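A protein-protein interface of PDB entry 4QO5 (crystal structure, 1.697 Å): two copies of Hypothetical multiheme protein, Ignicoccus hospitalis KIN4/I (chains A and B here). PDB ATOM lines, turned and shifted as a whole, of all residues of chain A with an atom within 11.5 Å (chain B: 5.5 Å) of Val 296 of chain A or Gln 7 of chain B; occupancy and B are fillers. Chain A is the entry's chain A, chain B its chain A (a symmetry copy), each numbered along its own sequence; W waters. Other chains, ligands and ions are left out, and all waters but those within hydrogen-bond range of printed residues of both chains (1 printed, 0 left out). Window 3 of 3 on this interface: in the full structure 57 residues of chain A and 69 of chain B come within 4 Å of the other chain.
OG1 of Thr 297 of chain A lies close to N of Glu 299 of chain A (3.2 Å). N of Gln 7 of chain B is in hydrogen-bond range of OD1 of Asn 5 of chain B (3.2 Å). The side-chain amide oxygen of Asn 294 of chain A is in hydrogen-bond range of the backbone NH of Val 296 of chain A (2.9 Å). The backbone carbonyl oxygen (O) of Glu 299 of chain A is in hydrogen-bond range of the backbone NH (N) of Asn 294 of chain A, 2.8 Å away. The side-chain amide oxygen (OD1) of Asn 294 of chain A lies within hydrogen-bond range of the backbone NH (N) of Thr 297 of chain A, at 2.9 Å.
Of the printed residues of chain B, Val 296 of chain A touches Gln 7 and Ile 28. Gln 7 of chain B touches one residue of chain A. No residue of chain A comes within 4 Å of Asn 5 of chain B. Printed residues of chain A within 4 Å of Leu 6 of chain B: Pro 295. No residue of chain A comes within 4 Å of Glu 8 of chain B. No residue of chain A comes within 4 Å of Ala 9 of chain B. No residue of chain A comes within 4 Å of Val 10 of chain B. Ala 11 of chain B touches none of the printed residues of chain A. Ser 29 of chain B touches just these residues of chain A: Asn 294 (2.9 Å) and Thr 297 (3.8 Å). Of the printed residues of chain B, Pro 295 of chain A touches Leu 6. Of the printed residues of chain B, Asn 294 of chain A touches Ser 29. Printed residues of chain B within 4 Å of Thr 297 of chain A: Ser 29. The nearest residue of chain B that does not touch Val 296 of chain A is Ser 29 of chain B (4.1 Å). The nearest printed residue of chain B that does not touch Pro 295 of chain A is Gln 7 of chain B (5.3 Å).
No position is printed for both chains. Of the 5 pairs that touch across the chains among the printed residues, none has its exchanged pair printed and touching as well.
Of the 10 printed residues of chain B, 4 touch a printed residue of chain A. Among the printed residues, no Asp or Glu carboxylate lies within 4 Å of a Lys or Arg side-chain nitrogen of the other chain.
Water W1 lies within hydrogen-bond range of O of Val 296 of chain A (2.6 Å) and OE1 of Gln 7 of chain B (3.2 Å).
The side-chain amide nitrogen (ND2) of Asn 294 of chain A is in hydrogen-bond range of the backbone carbonyl oxygen (O) of Ser 29 of chain B.
Among the printed residues, merely in contact across the chains: Pro 295 of chain A with Leu 6 of chain B, Val 296 of chain A with Gln 7 of chain B, Val 296 of chain A with Ile 28 of chain B and Thr 297 of chain A with Ser 29 of chain B.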
ATOM      1  N   LEU A  57      -4.383  33.259  -7.076  1.00  0.00           N
ATOM      2  CA  LEU A  57      -3.595  32.197  -7.709  1.00  0.00           C
ATOM      3  C   LEU A  57      -4.199  31.661  -9.012  1.00  0.00           C
ATOM      4  O   LEU A  57      -3.482  31.191  -9.893  1.00  0.00           O
ATOM      5  CB  LEU A  57      -3.377  31.040  -6.726  1.00  0.00           C
ATOM      6  CG  LEU A  57      -2.362  31.293  -5.612  1.00  0.00           C
ATOM      7  CD1 LEU A  57      -2.222  30.058  -4.743  1.00  0.00           C
ATOM      8  CD2 LEU A  57      -1.010  31.706  -6.185  1.00  0.00           C
ATOM      9  N   ALA A 272      -2.794  27.808 -11.750  1.00  0.00           N
ATOM     10  CA  ALA A 272      -1.734  27.574 -10.772  1.00  0.00           C
ATOM     11  C   ALA A 272      -1.301  26.108 -10.893  1.00  0.00           C
ATOM     12  O   ALA A 272      -2.038  25.213 -10.490  1.00  0.00           O
ATOM     13  CB  ALA A 272      -2.195  27.917  -9.358  1.00  0.00           C
ATOM     14  N   TRP A 273      -0.120  25.894 -11.483  1.00  0.00           N
ATOM     15  CA  TRP A 273       0.354  24.551 -11.908  1.00  0.00           C
ATOM     16  C   TRP A 273       0.794  23.773 -10.700  1.00  0.00           C
ATOM     17  O   TRP A 273       1.545  24.293  -9.898  1.00  0.00           O
ATOM     18  CB  TRP A 273       1.504  24.690 -12.964  1.00  0.00           C
ATOM     19  CG  TRP A 273       1.445  23.762 -14.084  1.00  0.00           C
ATOM     20  CD1 TRP A 273       2.415  23.066 -14.742  1.00  0.00           C
ATOM     21  CD2 TRP A 273       0.251  23.332 -14.572  1.00  0.00           C
ATOM     22  NE1 TRP A 273       1.815  22.245 -15.708  1.00  0.00           N
ATOM     23  CE2 TRP A 273       0.476  22.409 -15.572  1.00  0.00           C
ATOM     24  CE3 TRP A 273      -1.063  23.754 -14.353  1.00  0.00           C
ATOM     25  CZ2 TRP A 273      -0.478  22.012 -16.322  1.00  0.00           C
ATOM     26  CZ3 TRP A 273      -2.000  23.284 -15.054  1.00  0.00           C
ATOM     27  CH2 TRP A 273      -1.749  22.488 -16.020  1.00  0.00           C
ATOM     28  N   LYS A 274       0.286  22.557 -10.539  1.00  0.00           N
ATOM     29  CA  LYS A 274       0.615  21.795  -9.330  1.00  0.00           C
ATOM     30  C   LYS A 274       1.411  20.543  -9.646  1.00  0.00           C
ATOM     31  O   LYS A 274       0.859  19.590 -10.199  1.00  0.00           O
ATOM     32  CB  LYS A 274      -0.658  21.407  -8.561  1.00  0.00           C
ATOM     33  CG  LYS A 274      -1.508  22.604  -8.119  1.00  0.00           C
ATOM     34  CD  LYS A 274      -2.826  22.148  -7.482  1.00  0.00           C
ATOM     35  CE  LYS A 274      -3.741  21.448  -8.492  1.00  0.00           C
ATOM     36  NZ  LYS A 274      -4.136  22.335  -9.640  1.00  0.00           N
ATOM     37  N   PRO A 275       2.713  20.529  -9.287  1.00  0.00           N
ATOM     38  CA  PRO A 275       3.531  19.320  -9.492  1.00  0.00           C
ATOM     39  C   PRO A 275       2.870  18.121  -8.835  1.00  0.00           C
ATOM     40  O   PRO A 275       2.333  18.240  -7.740  1.00  0.00           O
ATOM     41  CB  PRO A 275       4.850  19.658  -8.787  1.00  0.00           C
ATOM     42  CG  PRO A 275       4.914  21.194  -8.841  1.00  0.00           C
ATOM     43  CD  PRO A 275       3.481  21.625  -8.659  1.00  0.00           C
ATOM     44  N   GLY A 276       2.887  16.974  -9.506  1.00  0.00           N
ATOM     45  CA  GLY A 276       2.292  15.784  -8.931  1.00  0.00           C
ATOM     46  C   GLY A 276       0.810  15.715  -9.239  1.00  0.00           C
ATOM     47  O   GLY A 276       0.358  14.830  -9.970  1.00  0.00           O
ATOM     48  N   ALA A 277       0.054  16.667  -8.711  1.00  0.00           N
ATOM     49  CA  ALA A 277      -1.393  16.683  -8.882  1.00  0.00           C
ATOM     50  C   ALA A 277      -1.761  16.885 -10.360  1.00  0.00           C
ATOM     51  O   ALA A 277      -2.683  16.232 -10.862  1.00  0.00           O
ATOM     52  CB  ALA A 277      -2.025  17.778  -8.020  1.00  0.00           C
ATOM     53  N   ASP A 278      -1.024  17.771 -11.036  1.00  0.00           N
ATOM     54  CA  ASP A 278      -1.320  18.166 -12.431  1.00  0.00           C
ATOM     55  C   ASP A 278      -0.376  17.532 -13.448  1.00  0.00           C
ATOM     56  O   ASP A 278      -0.717  17.423 -14.622  1.00  0.00           O
ATOM     57  CB  ASP A 278      -1.260  19.704 -12.600  1.00  0.00           C
ATOM     58  CG  ASP A 278      -2.351  20.424 -11.842  1.00  0.00           C
ATOM     59  OD1 ASP A 278      -3.411  19.800 -11.590  1.00  0.00           O
ATOM     60  OD2 ASP A 278      -2.158  21.629 -11.522  1.00  0.00           O
ATOM     61  N   LEU A 292       4.172  27.645 -10.021  1.00  0.00           N
ATOM     62  CA  LEU A 292       4.096  26.285  -9.480  1.00  0.00           C
ATOM     63  C   LEU A 292       3.676  26.347  -8.017  1.00  0.00           C
ATOM     64  O   LEU A 292       4.252  27.105  -7.233  1.00  0.00           O
ATOM     65  CB  LEU A 292       5.446  25.581  -9.597  1.00  0.00           C
ATOM     66  CG  LEU A 292       6.016  25.343 -11.003  1.00  0.00           C
ATOM     67  CD1 LEU A 292       7.324  24.554 -10.879  1.00  0.00           C
ATOM     68  CD2 LEU A 292       5.034  24.645 -11.996  1.00  0.00           C
ATOM     69  N   VAL A 293       2.653  25.575  -7.662  1.00  0.00           N
ATOM     70  CA  VAL A 293       2.110  25.589  -6.305  1.00  0.00           C
ATOM     71  C   VAL A 293       2.040  24.167  -5.742  1.00  0.00           C
ATOM     72  O   VAL A 293       1.633  23.225  -6.444  1.00  0.00           O
ATOM     73  CB  VAL A 293       0.701  26.238  -6.278  1.00  0.00           C
ATOM     74  CG1 VAL A 293       0.133  26.262  -4.868  1.00  0.00           C
ATOM     75  CG2 VAL A 293       0.765  27.661  -6.814  1.00  0.00           C
ATOM     76  N   ASN A 294       2.444  24.001  -4.481  1.00  0.00           N
ATOM     77  CA  ASN A 294       2.371  22.686  -3.850  1.00  0.00           C
ATOM     78  C   ASN A 294       0.909  22.269  -3.649  1.00  0.00           C
ATOM     79  O   ASN A 294       0.130  23.009  -3.052  1.00  0.00           O
ATOM     80  CB  ASN A 294       3.121  22.700  -2.519  1.00  0.00           C
ATOM     81  CG  ASN A 294       3.218  21.326  -1.893  1.00  0.00           C
ATOM     82  OD1 ASN A 294       2.214  20.744  -1.479  1.00  0.00           O
ATOM     83  ND2 ASN A 294       4.434  20.806  -1.805  1.00  0.00           N
ATOM     84  N   PRO A 295       0.532  21.078  -4.157  1.00  0.00           N
ATOM     85  CA  PRO A 295      -0.881  20.670  -4.169  1.00  0.00           C
ATOM     86  C   PRO A 295      -1.457  20.388  -2.796  1.00  0.00           C
ATOM     87  O   PRO A 295      -2.680  20.418  -2.620  1.00  0.00           O
ATOM     88  CB  PRO A 295      -0.871  19.381  -5.010  1.00  0.00           C
ATOM     89  CG  PRO A 295       0.539  18.898  -4.967  1.00  0.00           C
ATOM     90  CD  PRO A 295       1.382  20.144  -4.913  1.00  0.00           C
ATOM     91  N   VAL A 296      -0.584  20.122  -1.833  1.00  0.00           N
ATOM     92  CA  VAL A 296      -1.008  19.785  -0.485  1.00  0.00           C
ATOM     93  C   VAL A 296      -0.882  20.960   0.489  1.00  0.00           C
ATOM     94  O   VAL A 296      -1.775  21.195   1.312  1.00  0.00           O
ATOM     95  CB  VAL A 296      -0.206  18.569   0.028  1.00  0.00           C
ATOM     96  CG1 VAL A 296      -0.484  18.308   1.504  1.00  0.00           C
ATOM     97  CG2 VAL A 296      -0.532  17.355  -0.834  1.00  0.00           C
ATOM     98  N   THR A 297       0.218  21.699   0.396  1.00  0.00           N
ATOM     99  CA  THR A 297       0.468  22.788   1.344  1.00  0.00           C
ATOM    100  C   THR A 297       0.011  24.152   0.839  1.00  0.00           C
ATOM    101  O   THR A 297      -0.204  25.068   1.634  1.00  0.00           O
ATOM    102  CB  THR A 297       1.954  22.889   1.722  1.00  0.00           C
ATOM    103  OG1 THR A 297       2.694  23.374   0.598  1.00  0.00           O
ATOM    104  CG2 THR A 297       2.500  21.524   2.148  1.00  0.00           C
ATOM    105  N   GLY A 298      -0.131  24.302  -0.474  1.00  0.00           N
ATOM    106  CA  GLY A 298      -0.514  25.592  -1.026  1.00  0.00           C
ATOM    107  C   GLY A 298       0.665  26.537  -1.175  1.00  0.00           C
ATOM    108  O   GLY A 298       0.520  27.637  -1.692  1.00  0.00           O
ATOM    109  N   GLU A 299       1.836  26.112  -0.717  1.00  0.00           N
ATOM    110  CA  GLU A 299       3.052  26.915  -0.846  1.00  0.00           C
ATOM    111  C   GLU A 299       3.390  27.184  -2.310  1.00  0.00           C
ATOM    112  O   GLU A 299       3.366  26.273  -3.143  1.00  0.00           O
ATOM    113  CB  GLU A 299       4.237  26.201  -0.189  1.00  0.00           C
ATOM    114  CG  GLU A 299       5.578  26.906  -0.390  1.00  0.00           C
ATOM    115  CD  GLU A 299       6.769  26.077   0.083  1.00  0.00           C
ATOM    116  OE1 GLU A 299       6.711  24.830  -0.003  1.00  0.00           O
ATOM    117  OE2 GLU A 299       7.767  26.677   0.538  1.00  0.00           O
ATOM    118  N   VAL A 300       3.721  28.430  -2.625  1.00  0.00           N
ATOM    119  CA  VAL A 300       4.224  28.745  -3.954  1.00  0.00           C
ATOM    120  C   VAL A 300       5.643  28.210  -4.093  1.00  0.00           C
ATOM    121  O   VAL A 300       6.538  28.592  -3.347  1.00  0.00           O
ATOM    122  CB  VAL A 300       4.193  30.260  -4.235  1.00  0.00           C
ATOM    123  CG1 VAL A 300       4.857  30.574  -5.581  1.00  0.00           C
ATOM    124  CG2 VAL A 300       2.764  30.755  -4.230  1.00  0.00           C
ATOM    125  N   ILE A 301       5.836  27.296  -5.034  1.00  0.00           N
ATOM    126  CA  ILE A 301       7.146  26.726  -5.310  1.00  0.00           C
ATOM    127  C   ILE A 301       7.956  27.647  -6.213  1.00  0.00           C
ATOM    128  O   ILE A 301       9.168  27.810  -6.046  1.00  0.00           O
ATOM    129  CB  ILE A 301       6.985  25.340  -5.976  1.00  0.00           C
ATOM    130  CG1 ILE A 301       6.368  24.348  -4.983  1.00  0.00           C
ATOM    131  CG2 ILE A 301       8.325  24.827  -6.530  1.00  0.00           C
ATOM    132  CD1 ILE A 301       5.885  23.046  -5.660  1.00  0.00           C
ATOM    133  N   ALA A 409      10.368  19.211  -5.996  1.00  0.00           N
ATOM    134  CA  ALA A 409       9.005  18.698  -6.033  1.00  0.00           C
ATOM    135  C   ALA A 409       9.010  17.214  -6.383  1.00  0.00           C
ATOM    136  O   ALA A 409       8.079  16.487  -6.024  1.00  0.00           O
ATOM    137  CB  ALA A 409       8.157  19.475  -7.037  1.00  0.00           C
ATOM    138  N   ASN B   5      -6.366  14.549  -6.839  1.00  0.00           N
ATOM    139  CA  ASN B   5      -6.350  14.934  -5.428  1.00  0.00           C
ATOM    140  C   ASN B   5      -5.513  13.900  -4.669  1.00  0.00           C
ATOM    141  O   ASN B   5      -5.979  12.790  -4.395  1.00  0.00           O
ATOM    142  CB  ASN B   5      -7.773  15.003  -4.873  1.00  0.00           C
ATOM    143  CG  ASN B   5      -7.820  15.459  -3.420  1.00  0.00           C
ATOM    144  OD1 ASN B   5      -6.958  15.116  -2.607  1.00  0.00           O
ATOM    145  ND2 ASN B   5      -8.839  16.242  -3.091  1.00  0.00           N
ATOM    146  N   LEU B   6      -4.275  14.264  -4.346  1.00  0.00           N
ATOM    147  CA  LEU B   6      -3.316  13.304  -3.809  1.00  0.00           C
ATOM    148  C   LEU B   6      -3.722  12.731  -2.454  1.00  0.00           C
ATOM    149  O   LEU B   6      -3.521  11.540  -2.189  1.00  0.00           O
ATOM    150  CB  LEU B   6      -1.914  13.912  -3.744  1.00  0.00           C
ATOM    151  CG  LEU B   6      -1.359  14.331  -5.106  1.00  0.00           C
ATOM    152  CD1 LEU B   6      -0.001  14.975  -4.964  1.00  0.00           C
ATOM    153  CD2 LEU B   6      -1.272  13.106  -6.013  1.00  0.00           C
ATOM    154  N   GLN B   7      -4.293  13.571  -1.601  1.00  0.00           N
ATOM    155  CA  GLN B   7      -4.701  13.125  -0.274  1.00  0.00           C
ATOM    156  C   GLN B   7      -5.835  12.110  -0.371  1.00  0.00           C
ATOM    157  O   GLN B   7      -5.830  11.087   0.323  1.00  0.00           O
ATOM    158  CB  GLN B   7      -5.097  14.320   0.597  1.00  0.00           C
ATOM    159  CG  GLN B   7      -3.897  15.075   1.136  1.00  0.00           C
ATOM    160  CD  GLN B   7      -4.253  16.440   1.682  1.00  0.00           C
ATOM    161  OE1 GLN B   7      -4.909  17.236   1.014  1.00  0.00           O
ATOM    162  NE2 GLN B   7      -3.821  16.717   2.911  1.00  0.00           N
ATOM    163  N   GLU B   8      -6.791  12.383  -1.254  1.00  0.00           N
ATOM    164  CA  GLU B   8      -7.913  11.479  -1.432  1.00  0.00           C
ATOM    165  C   GLU B   8      -7.448  10.168  -2.076  1.00  0.00           C
ATOM    166  O   GLU B   8      -7.937   9.095  -1.730  1.00  0.00           O
ATOM    167  CB  GLU B   8      -9.026  12.134  -2.257  1.00  0.00           C
ATOM    168  CG  GLU B   8      -9.939  11.138  -2.942  1.00  0.00           C
ATOM    169  CD  GLU B   8     -11.407  11.448  -2.725  1.00  0.00           C
ATOM    170  OE1 GLU B   8     -11.850  12.551  -3.121  1.00  0.00           O
ATOM    171  OE2 GLU B   8     -12.113  10.593  -2.142  1.00  0.00           O
ATOM    172  N   ALA B   9      -6.486  10.259  -2.992  1.00  0.00           N
ATOM    173  CA  ALA B   9      -5.981   9.074  -3.672  1.00  0.00           C
ATOM    174  C   ALA B   9      -5.223   8.178  -2.697  1.00  0.00           C
ATOM    175  O   ALA B   9      -5.331   6.950  -2.756  1.00  0.00           O
ATOM    176  CB  ALA B   9      -5.090   9.466  -4.850  1.00  0.00           C
ATOM    177  N   VAL B  10      -4.451   8.784  -1.805  1.00  0.00           N
ATOM    178  CA  VAL B  10      -3.748   8.002  -0.785  1.00  0.00           C
ATOM    179  C   VAL B  10      -4.720   7.317   0.184  1.00  0.00           C
ATOM    180  O   VAL B  10      -4.541   6.143   0.544  1.00  0.00           O
ATOM    181  CB  VAL B  10      -2.717   8.855  -0.029  1.00  0.00           C
ATOM    182  CG1 VAL B  10      -2.237   8.136   1.240  1.00  0.00           C
ATOM    183  CG2 VAL B  10      -1.535   9.161  -0.946  1.00  0.00           C
ATOM    184  N   ALA B  11      -5.763   8.045   0.577  1.00  0.00           N
ATOM    185  CA  ALA B  11      -6.760   7.532   1.518  1.00  0.00           C
ATOM    186  C   ALA B  11      -7.560   6.351   0.959  1.00  0.00           C
ATOM    187  O   ALA B  11      -8.054   5.517   1.718  1.00  0.00           O
ATOM    188  CB  ALA B  11      -7.704   8.645   1.943  1.00  0.00           C
ATOM    189  N   LYS B  12      -7.693   6.293  -0.361  1.00  0.00           N
ATOM    190  CA  LYS B  12      -8.453   5.231  -1.013  1.00  0.00           C
ATOM    191  C   LYS B  12      -7.627   3.965  -1.251  1.00  0.00           C
ATOM    192  O   LYS B  12      -8.170   2.937  -1.646  1.00  0.00           O
ATOM    193  CB  LYS B  12      -9.039   5.713  -2.349  1.00  0.00           C
ATOM    194  CG  LYS B  12     -10.451   6.302  -2.252  1.00  0.00           C
ATOM    195  CD  LYS B  12     -11.153   5.879  -0.955  1.00  0.00           C
ATOM    196  CE  LYS B  12     -12.634   6.258  -0.945  1.00  0.00           C
ATOM    197  NZ  LYS B  12     -13.442   5.444  -1.899  1.00  0.00           N
ATOM    198  N   ILE B  28       3.994  13.096   0.651  1.00  0.00           N
ATOM    199  CA  ILE B  28       2.921  13.685  -0.146  1.00  0.00           C
ATOM    200  C   ILE B  28       3.076  15.214  -0.184  1.00  0.00           C
ATOM    201  O   ILE B  28       2.723  15.866  -1.171  1.00  0.00           O
ATOM    202  CB  ILE B  28       1.532  13.257   0.385  1.00  0.00           C
ATOM    203  CG1 ILE B  28       0.440  13.544  -0.646  1.00  0.00           C
ATOM    204  CG2 ILE B  28       1.218  13.916   1.726  1.00  0.00           C
ATOM    205  CD1 ILE B  28      -0.912  12.970  -0.240  1.00  0.00           C
ATOM    206  N   SER B  29       3.645  15.786   0.870  1.00  0.00           N
ATOM    207  CA  SER B  29       3.862  17.233   0.882  1.00  0.00           C
ATOM    208  C   SER B  29       5.283  17.634   0.464  1.00  0.00           C
ATOM    209  O   SER B  29       5.475  18.695  -0.116  1.00  0.00           O
ATOM    210  CB  SER B  29       3.490  17.840   2.240  1.00  0.00           C
ATOM    211  OG  SER B  29       4.408  17.466   3.245  1.00  0.00           O
HETATM  212  O   HOH W   1      -4.143  20.221   1.854  1.00  0.00           O
